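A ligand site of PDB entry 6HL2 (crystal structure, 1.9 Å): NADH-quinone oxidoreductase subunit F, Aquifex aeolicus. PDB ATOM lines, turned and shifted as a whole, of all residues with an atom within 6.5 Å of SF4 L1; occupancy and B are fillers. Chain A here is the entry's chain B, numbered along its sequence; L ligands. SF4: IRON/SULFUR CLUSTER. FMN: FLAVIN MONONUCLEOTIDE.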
ATOM      1  N   ILE A 181     -28.617  -2.524   4.138  1.00  0.00           N
ATOM      2  CA  ILE A 181     -27.185  -2.327   4.074  1.00  0.00           C
ATOM      3  C   ILE A 181     -26.543  -3.027   2.862  1.00  0.00           C
ATOM      4  O   ILE A 181     -25.477  -2.606   2.425  1.00  0.00           O
ATOM      5  CB  ILE A 181     -26.496  -2.693   5.428  1.00  0.00           C
ATOM      6  CG1 ILE A 181     -25.081  -2.111   5.508  1.00  0.00           C
ATOM      7  CG2 ILE A 181     -26.472  -4.227   5.654  1.00  0.00           C
ATOM      8  CD1 ILE A 181     -24.999  -0.552   5.302  1.00  0.00           C
ATOM      9  N   GLU A 184     -25.153  -0.995  -0.036  1.00  0.00           N
ATOM     10  CA  GLU A 184     -23.830  -0.353   0.067  1.00  0.00           C
ATOM     11  C   GLU A 184     -22.897  -1.265  -0.704  1.00  0.00           C
ATOM     12  O   GLU A 184     -22.927  -2.479  -0.507  1.00  0.00           O
ATOM     13  CB  GLU A 184     -23.391  -0.212   1.555  1.00  0.00           C
ATOM     14  CG  GLU A 184     -22.227   0.744   1.743  1.00  0.00           C
ATOM     15  CD  GLU A 184     -20.833   0.193   1.513  1.00  0.00           C
ATOM     16  OE1 GLU A 184     -20.674  -1.050   1.546  1.00  0.00           O
ATOM     17  OE2 GLU A 184     -19.890   0.989   1.367  1.00  0.00           O
ATOM     18  N   HIS A 198     -21.825  -7.178   5.492  1.00  0.00           N
ATOM     19  CA  HIS A 198     -21.106  -6.256   6.355  1.00  0.00           C
ATOM     20  C   HIS A 198     -20.188  -5.364   5.531  1.00  0.00           C
ATOM     21  O   HIS A 198     -19.262  -5.874   4.901  1.00  0.00           O
ATOM     22  CB  HIS A 198     -20.297  -7.020   7.418  1.00  0.00           C
ATOM     23  CG  HIS A 198     -21.107  -7.575   8.548  1.00  0.00           C
ATOM     24  ND1 HIS A 198     -20.604  -8.542   9.380  1.00  0.00           N
ATOM     25  CD2 HIS A 198     -22.380  -7.296   8.931  1.00  0.00           C
ATOM     26  CE1 HIS A 198     -21.551  -8.815  10.253  1.00  0.00           C
ATOM     27  NE2 HIS A 198     -22.634  -8.075  10.040  1.00  0.00           N
ATOM     28  N   PRO A 199     -20.407  -4.024   5.508  1.00  0.00           N
ATOM     29  CA  PRO A 199     -19.503  -3.157   4.745  1.00  0.00           C
ATOM     30  C   PRO A 199     -18.036  -3.288   5.147  1.00  0.00           C
ATOM     31  O   PRO A 199     -17.719  -3.550   6.312  1.00  0.00           O
ATOM     32  CB  PRO A 199     -20.036  -1.751   5.033  1.00  0.00           C
ATOM     33  CG  PRO A 199     -21.485  -1.972   5.312  1.00  0.00           C
ATOM     34  CD  PRO A 199     -21.510  -3.240   6.110  1.00  0.00           C
ATOM     35  N   ARG A 200     -17.154  -3.130   4.167  1.00  0.00           N
ATOM     36  CA  ARG A 200     -15.710  -3.197   4.374  1.00  0.00           C
ATOM     37  C   ARG A 200     -15.150  -1.789   4.372  1.00  0.00           C
ATOM     38  O   ARG A 200     -15.664  -0.901   3.685  1.00  0.00           O
ATOM     39  CB  ARG A 200     -15.027  -3.987   3.238  1.00  0.00           C
ATOM     40  CG  ARG A 200     -15.522  -5.412   3.023  1.00  0.00           C
ATOM     41  CD  ARG A 200     -14.502  -6.238   2.227  1.00  0.00           C
ATOM     42  NE  ARG A 200     -13.283  -6.502   3.013  1.00  0.00           N
ATOM     43  CZ  ARG A 200     -13.134  -7.518   3.861  1.00  0.00           C
ATOM     44  NH1 ARG A 200     -14.102  -8.402   4.027  1.00  0.00           N
ATOM     45  NH2 ARG A 200     -12.001  -7.662   4.537  1.00  0.00           N
ATOM     46  N   GLU A 345     -31.907  -1.008  10.300  1.00  0.00           N
ATOM     47  CA  GLU A 345     -30.963  -1.343   9.239  1.00  0.00           C
ATOM     48  C   GLU A 345     -29.455  -1.241   9.577  1.00  0.00           C
ATOM     49  O   GLU A 345     -28.649  -1.708   8.772  1.00  0.00           O
ATOM     50  CB  GLU A 345     -31.278  -0.511   7.986  1.00  0.00           C
ATOM     51  CG  GLU A 345     -32.687  -0.752   7.454  1.00  0.00           C
ATOM     52  CD  GLU A 345     -33.129  -2.170   7.094  1.00  0.00           C
ATOM     53  OE1 GLU A 345     -32.276  -3.073   6.932  1.00  0.00           O
ATOM     54  OE2 GLU A 345     -34.352  -2.355   6.919  1.00  0.00           O
ATOM     55  N   THR A 346     -29.077  -0.677  10.736  1.00  0.00           N
ATOM     56  CA  THR A 346     -27.639  -0.653  11.070  1.00  0.00           C
ATOM     57  C   THR A 346     -27.106  -2.092  11.155  1.00  0.00           C
ATOM     58  O   THR A 346     -27.775  -2.940  11.724  1.00  0.00           O
ATOM     59  CB  THR A 346     -27.342   0.158  12.331  1.00  0.00           C
ATOM     60  OG1 THR A 346     -25.965  -0.049  12.683  1.00  0.00           O
ATOM     61  CG2 THR A 346     -28.241  -0.225  13.518  1.00  0.00           C
ATOM     62  N   CYS A 347     -25.930  -2.376  10.551  1.00  0.00           N
ATOM     63  CA  CYS A 347     -25.385  -3.740  10.633  1.00  0.00           C
ATOM     64  C   CYS A 347     -24.722  -3.996  11.992  1.00  0.00           C
ATOM     65  O   CYS A 347     -24.405  -5.132  12.330  1.00  0.00           O
ATOM     66  CB  CYS A 347     -24.454  -4.034   9.459  1.00  0.00           C
ATOM     67  SG  CYS A 347     -22.808  -3.295   9.627  1.00  0.00           S
ATOM     68  N   GLY A 348     -24.464  -2.924  12.742  1.00  0.00           N
ATOM     69  CA  GLY A 348     -23.894  -3.009  14.095  1.00  0.00           C
ATOM     70  C   GLY A 348     -22.399  -3.212  14.251  1.00  0.00           C
ATOM     71  O   GLY A 348     -21.939  -3.399  15.387  1.00  0.00           O
ATOM     72  N   GLN A 349     -21.618  -3.139  13.160  1.00  0.00           N
ATOM     73  CA  GLN A 349     -20.148  -3.340  13.206  1.00  0.00           C
ATOM     74  C   GLN A 349     -19.438  -2.225  13.960  1.00  0.00           C
ATOM     75  O   GLN A 349     -18.430  -2.459  14.645  1.00  0.00           O
ATOM     76  CB  GLN A 349     -19.556  -3.354  11.769  1.00  0.00           C
ATOM     77  CG  GLN A 349     -19.746  -4.649  10.991  1.00  0.00           C
ATOM     78  CD  GLN A 349     -18.876  -4.613   9.758  1.00  0.00           C
ATOM     79  OE1 GLN A 349     -17.749  -5.143   9.761  1.00  0.00           O
ATOM     80  NE2 GLN A 349     -19.310  -3.911   8.719  1.00  0.00           N
ATOM     81  N   CYS A 350     -19.969  -0.994  13.801  1.00  0.00           N
ATOM     82  CA  CYS A 350     -19.412   0.212  14.408  1.00  0.00           C
ATOM     83  C   CYS A 350     -20.260   0.552  15.634  1.00  0.00           C
ATOM     84  O   CYS A 350     -21.498   0.608  15.542  1.00  0.00           O
ATOM     85  CB  CYS A 350     -19.414   1.351  13.387  1.00  0.00           C
ATOM     86  SG  CYS A 350     -18.850   0.844  11.734  1.00  0.00           S
ATOM     87  N   THR A 351     -19.623   0.769  16.771  1.00  0.00           N
ATOM     88  CA  THR A 351     -20.297   1.042  18.047  1.00  0.00           C
ATOM     89  C   THR A 351     -21.172   2.301  18.002  1.00  0.00           C
ATOM     90  O   THR A 351     -22.345   2.164  18.323  1.00  0.00           O
ATOM     91  CB  THR A 351     -19.280   1.040  19.199  1.00  0.00           C
ATOM     92  OG1 THR A 351     -18.764  -0.289  19.307  1.00  0.00           O
ATOM     93  CG2 THR A 351     -19.913   1.471  20.550  1.00  0.00           C
ATOM     94  N   CYS A 353     -22.575   3.812  15.534  1.00  0.00           N
ATOM     95  CA  CYS A 353     -23.689   3.552  14.636  1.00  0.00           C
ATOM     96  C   CYS A 353     -24.683   2.581  15.282  1.00  0.00           C
ATOM     97  O   CYS A 353     -25.885   2.863  15.292  1.00  0.00           O
ATOM     98  CB  CYS A 353     -23.221   3.048  13.268  1.00  0.00           C
ATOM     99  SG  CYS A 353     -24.571   2.801  12.082  1.00  0.00           S
ATOM    100  N   ARG A 354     -24.175   1.449  15.819  1.00  0.00           N
ATOM    101  CA  ARG A 354     -24.980   0.399  16.453  1.00  0.00           C
ATOM    102  C   ARG A 354     -25.832   0.982  17.592  1.00  0.00           C
ATOM    103  O   ARG A 354     -27.057   0.848  17.585  1.00  0.00           O
ATOM    104  CB  ARG A 354     -24.059  -0.716  17.034  1.00  0.00           C
ATOM    105  CG  ARG A 354     -24.785  -1.850  17.761  1.00  0.00           C
ATOM    106  CD  ARG A 354     -23.831  -2.947  18.250  1.00  0.00           C
ATOM    107  NE  ARG A 354     -22.944  -2.487  19.337  1.00  0.00           N
ATOM    108  CZ  ARG A 354     -21.647  -2.231  19.183  1.00  0.00           C
ATOM    109  NH1 ARG A 354     -21.061  -2.373  17.997  1.00  0.00           N
ATOM    110  NH2 ARG A 354     -20.921  -1.817  20.221  1.00  0.00           N
ATOM    111  N   CYS A 357     -28.065   4.455  16.407  1.00  0.00           N
ATOM    112  CA  CYS A 357     -29.307   4.226  15.634  1.00  0.00           C
ATOM    113  C   CYS A 357     -30.383   3.661  16.554  1.00  0.00           C
ATOM    114  O   CYS A 357     -31.538   4.054  16.449  1.00  0.00           O
ATOM    115  CB  CYS A 357     -29.061   3.302  14.440  1.00  0.00           C
ATOM    116  SG  CYS A 357     -28.093   4.059  13.103  1.00  0.00           S
ATOM    117  N   ILE A 387     -23.818   9.528  15.899  1.00  0.00           N
ATOM    118  CA  ILE A 387     -23.951   8.220  15.259  1.00  0.00           C
ATOM    119  C   ILE A 387     -22.740   7.993  14.323  1.00  0.00           C
ATOM    120  O   ILE A 387     -22.277   6.855  14.154  1.00  0.00           O
ATOM    121  CB  ILE A 387     -25.316   8.112  14.492  1.00  0.00           C
ATOM    122  CG1 ILE A 387     -26.530   8.389  15.432  1.00  0.00           C
ATOM    123  CG2 ILE A 387     -25.463   6.755  13.813  1.00  0.00           C
ATOM    124  CD1 ILE A 387     -27.876   8.541  14.766  1.00  0.00           C
ATOM    125  N   GLN A 388     -22.256   9.080  13.704  1.00  0.00           N
ATOM    126  CA  GLN A 388     -21.191   9.074  12.689  1.00  0.00           C
ATOM    127  C   GLN A 388     -19.789   8.654  13.209  1.00  0.00           C
ATOM    128  O   GLN A 388     -19.106   7.944  12.473  1.00  0.00           O
ATOM    129  CB  GLN A 388     -21.122  10.442  11.975  1.00  0.00           C
ATOM    130  CG  GLN A 388     -20.130  10.528  10.810  1.00  0.00           C
ATOM    131  CD  GLN A 388     -20.413  11.656   9.851  1.00  0.00           C
ATOM    132  OE1 GLN A 388     -21.519  12.233   9.796  1.00  0.00           O
ATOM    133  NE2 GLN A 388     -19.426  11.988   9.028  1.00  0.00           N
ATOM    134  N   THR A 390     -16.324   7.051  13.895  1.00  0.00           N
ATOM    135  CA  THR A 390     -15.689   5.752  13.608  1.00  0.00           C
ATOM    136  C   THR A 390     -16.444   4.900  12.544  1.00  0.00           C
ATOM    137  O   THR A 390     -15.979   3.797  12.222  1.00  0.00           O
ATOM    138  CB  THR A 390     -15.409   4.937  14.900  1.00  0.00           C
ATOM    139  OG1 THR A 390     -16.581   4.206  15.264  1.00  0.00           O
ATOM    140  CG2 THR A 390     -14.910   5.798  16.071  1.00  0.00           C
ATOM    141  N   SER A 391     -17.587   5.369  12.029  1.00  0.00           N
ATOM    142  CA  SER A 391     -18.400   4.627  11.040  1.00  0.00           C
ATOM    143  C   SER A 391     -17.586   4.241   9.783  1.00  0.00           C
ATOM    144  O   SER A 391     -16.820   5.057   9.268  1.00  0.00           O
ATOM    145  CB  SER A 391     -19.661   5.403  10.679  1.00  0.00           C
ATOM    146  OG  SER A 391     -19.348   6.656  10.090  1.00  0.00           O
ATOM    147  N   ILE A 392     -17.696   2.977   9.344  1.00  0.00           N
ATOM    148  CA  ILE A 392     -17.044   2.406   8.154  1.00  0.00           C
ATOM    149  C   ILE A 392     -17.799   2.843   6.888  1.00  0.00           C
ATOM    150  O   ILE A 392     -17.197   2.885   5.822  1.00  0.00           O
ATOM    151  CB  ILE A 392     -17.078   0.841   8.196  1.00  0.00           C
ATOM    152  CG1 ILE A 392     -16.090   0.233   9.161  1.00  0.00           C
ATOM    153  CG2 ILE A 392     -16.905   0.191   6.781  1.00  0.00           C
ATOM    154  CD1 ILE A 392     -16.307  -1.322   9.298  1.00  0.00           C
ATOM    155  N   CYS A 393     -19.126   3.021   6.951  1.00  0.00           N
ATOM    156  CA  CYS A 393     -19.908   3.273   5.734  1.00  0.00           C
ATOM    157  C   CYS A 393     -20.828   4.488   5.851  1.00  0.00           C
ATOM    158  O   CYS A 393     -20.919   5.090   6.907  1.00  0.00           O
ATOM    159  CB  CYS A 393     -20.659   2.007   5.301  1.00  0.00           C
ATOM    160  SG  CYS A 393     -22.346   1.827   5.977  1.00  0.00           S
ATOM    161  N   GLY A 394     -21.497   4.828   4.740  1.00  0.00           N
ATOM    162  CA  GLY A 394     -22.384   5.975   4.641  1.00  0.00           C
ATOM    163  C   GLY A 394     -23.577   5.989   5.571  1.00  0.00           C
ATOM    164  O   GLY A 394     -24.066   7.058   5.892  1.00  0.00           O
ATOM    165  N   LEU A 395     -24.090   4.800   5.979  1.00  0.00           N
ATOM    166  CA  LEU A 395     -25.263   4.730   6.853  1.00  0.00           C
ATOM    167  C   LEU A 395     -25.073   5.489   8.182  1.00  0.00           C
ATOM    168  O   LEU A 395     -25.909   6.298   8.542  1.00  0.00           O
ATOM    169  CB  LEU A 395     -25.719   3.277   7.081  1.00  0.00           C
ATOM    170  CG  LEU A 395     -27.116   3.089   7.690  1.00  0.00           C
ATOM    171  CD1 LEU A 395     -27.709   1.758   7.270  1.00  0.00           C
ATOM    172  CD2 LEU A 395     -27.078   3.151   9.248  1.00  0.00           C
ATOM    173  N   GLY A 396     -23.958   5.217   8.872  1.00  0.00           N
ATOM    174  CA  GLY A 396     -23.635   5.881  10.126  1.00  0.00           C
ATOM    175  C   GLY A 396     -23.498   7.381   9.958  1.00  0.00           C
ATOM    176  O   GLY A 396     -23.940   8.144  10.817  1.00  0.00           O
ATOM    177  N   ALA A 397     -22.960   7.802   8.783  1.00  0.00           N
ATOM    178  CA  ALA A 397     -22.767   9.223   8.465  1.00  0.00           C
ATOM    179  C   ALA A 397     -24.076  10.000   8.246  1.00  0.00           C
ATOM    180  O   ALA A 397     -24.076  11.215   8.394  1.00  0.00           O
ATOM    181  CB  ALA A 397     -21.883   9.356   7.230  1.00  0.00           C
HETATM  182 FE1  SF4 L   1     -22.673  -1.082   9.730  1.00  0.00          FE
HETATM  183 FE2  SF4 L   1     -23.360   1.432  10.595  1.00  0.00          FE
HETATM  184 FE3  SF4 L   1     -22.118   1.124   8.188  1.00  0.00          FE
HETATM  185 FE4  SF4 L   1     -20.734   0.719  10.489  1.00  0.00          FE
HETATM  186  S1  SF4 L   1     -21.621   2.689   9.751  1.00  0.00           S
HETATM  187  S2  SF4 L   1     -20.661  -0.584   8.643  1.00  0.00           S
HETATM  188  S3  SF4 L   1     -22.401  -0.236  11.806  1.00  0.00           S
HETATM  189  S4  SF4 L   1     -24.202   0.368   8.792  1.00  0.00           S
HETATM  190  N1  FMN L   2     -26.673   2.387  -4.544  1.00  0.00           N
HETATM  191  C2  FMN L   2     -27.591   1.757  -5.315  1.00  0.00           C
HETATM  192  O2  FMN L   2     -27.423   1.663  -6.540  1.00  0.00           O
HETATM  193  N3  FMN L   2     -28.673   1.123  -4.714  1.00  0.00           N
HETATM  194  C4  FMN L   2     -28.910   1.041  -3.354  1.00  0.00           C
HETATM  195  O4  FMN L   2     -29.883   0.407  -2.935  1.00  0.00           O
HETATM  196  C4A FMN L   2     -27.901   1.676  -2.536  1.00  0.00           C
HETATM  197  N5  FMN L   2     -27.990   1.565  -1.235  1.00  0.00           N
HETATM  198  C5A FMN L   2     -26.980   2.095  -0.454  1.00  0.00           C
HETATM  199  C6  FMN L   2     -27.066   1.967   0.933  1.00  0.00           C
HETATM  200  C7  FMN L   2     -26.108   2.539   1.762  1.00  0.00           C
HETATM  201  C7M FMN L   2     -26.260   2.405   3.267  1.00  0.00           C
HETATM  202  C8  FMN L   2     -25.022   3.250   1.194  1.00  0.00           C
HETATM  203  C8M FMN L   2     -23.995   3.933   2.061  1.00  0.00           C
HETATM  204  C9  FMN L   2     -24.919   3.345  -0.191  1.00  0.00           C
HETATM  205  C9A FMN L   2     -25.884   2.787  -1.027  1.00  0.00           C
HETATM  206  N10 FMN L   2     -25.814   2.872  -2.441  1.00  0.00           N
HETATM  207  C10 FMN L   2     -26.805   2.330  -3.220  1.00  0.00           C
HETATM  208  C1' FMN L   2     -24.604   3.439  -3.060  1.00  0.00           C
HETATM  209  C2' FMN L   2     -23.625   2.350  -3.506  1.00  0.00           C
HETATM  210  O2' FMN L   2     -22.739   2.015  -2.440  1.00  0.00           O
HETATM  211  C3' FMN L   2     -22.846   2.777  -4.759  1.00  0.00           C
HETATM  212  O3' FMN L   2     -22.366   4.109  -4.573  1.00  0.00           O
HETATM  213  C4' FMN L   2     -23.607   2.719  -6.085  1.00  0.00           C
HETATM  214  O4' FMN L   2     -24.288   1.467  -6.231  1.00  0.00           O
HETATM  215  C5' FMN L   2     -22.665   2.928  -7.256  1.00  0.00           C
HETATM  216  O5' FMN L   2     -23.438   3.066  -8.481  1.00  0.00           O
HETATM  217  P   FMN L   2     -23.645   4.462  -9.211  1.00  0.00           P
HETATM  218  O1P FMN L   2     -24.534   5.360  -8.440  1.00  0.00           O
HETATM  219  O2P FMN L   2     -22.245   5.084  -9.409  1.00  0.00           O
HETATM  220  O3P FMN L   2     -24.190   4.090 -10.584  1.00  0.00           O
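Ile 181 touches SF4 L1 (CD1 to S4, 3.7 Å).
CG of Pro 199 touches S2 of SF4 L1, at 3.7 Å.
Ser 391 touches SF4 L1.
Ile 392 touches SF4 L1 (CB to S2, 3.9 Å).
Leu 395 touches SF4 L1.
Hydrophobic or aromatic side chains within 4 Å of SF4 L1: Ile 181, Pro 199, Ile 392 and Leu 395.
Of the 25 residues printed, 13 come within 4 Å of SF4 L1.
Along chain A the residues within 4 Å of SF4 L1 span positions 181 to 396.
The nearest printed residue that does not touch SF4 L1 is Arg 354 (4.7 Å).
The side-chain amide nitrogen (NE2) of Gln 349 sits close to the side-chain sulfur (SG) of Cys 347 (3.7 Å).
N of Leu 395 lies close to SG of Cys 393 (3.4 Å).
O of Cys 353 sits close to SG of Cys 357.
N of Cys 353 is in hydrogen-bond range of O of Ile 387 (3.4 Å).
The side-chain amide nitrogen (NE2) of Gln 349 sits at hydrogen-bond distance from the backbone carbonyl oxygen (O) of Pro 199 (2.9 Å).
N of Gly 348 sits close to OG1 of Thr 346, 3.2 Å away.
The backbone carbonyl oxygen (O) of Gly 348 sits at hydrogen-bond distance from the guanidinium group (NH1) of Arg 354 (2.9 Å).
O of Gly 396 sits close to N of Gln 388, 3.5 Å away.
A sulfur (S4) of SF4 L1 lies close to the backbone NH (N) of Cys 347, at 3.7 Å.
The side-chain sulfur (SG) of Cys 347 is bound to an iron atom (FE1) of SF4 L1.
S3 of SF4 L1 lies close to N of Cys 350, at 3.2 Å.
An iron atom (FE4) of SF4 L1 is bound by the side-chain sulfur (SG) of Cys 350.
The backbone NH (N) of Cys 393 sits close to a sulfur (S1) of SF4 L1, at 3.8 Å.
SG of Cys 393 binds FE3 of SF4 L1 (2.3 Å).
An iron atom (FE2) of SF4 L1 is bound by the side-chain sulfur (SG) of Cys 353 (2.4 Å).
N of Gln 349 lies close to S3 of SF4 L1, 3.3 Å away.
S2 of SF4 L1 lies close to NE2 of Gln 349, at 3.6 Å.
A sulfur (S3) of SF4 L1 lies close to the backbone NH (N) of Gly 348.
The backbone NH of Gly 396 sits close to a sulfur (S1) of SF4 L1, 3.6 Å away.
OG1 of Thr 346 sits close to S3 of SF4 L1 (3.7 Å).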
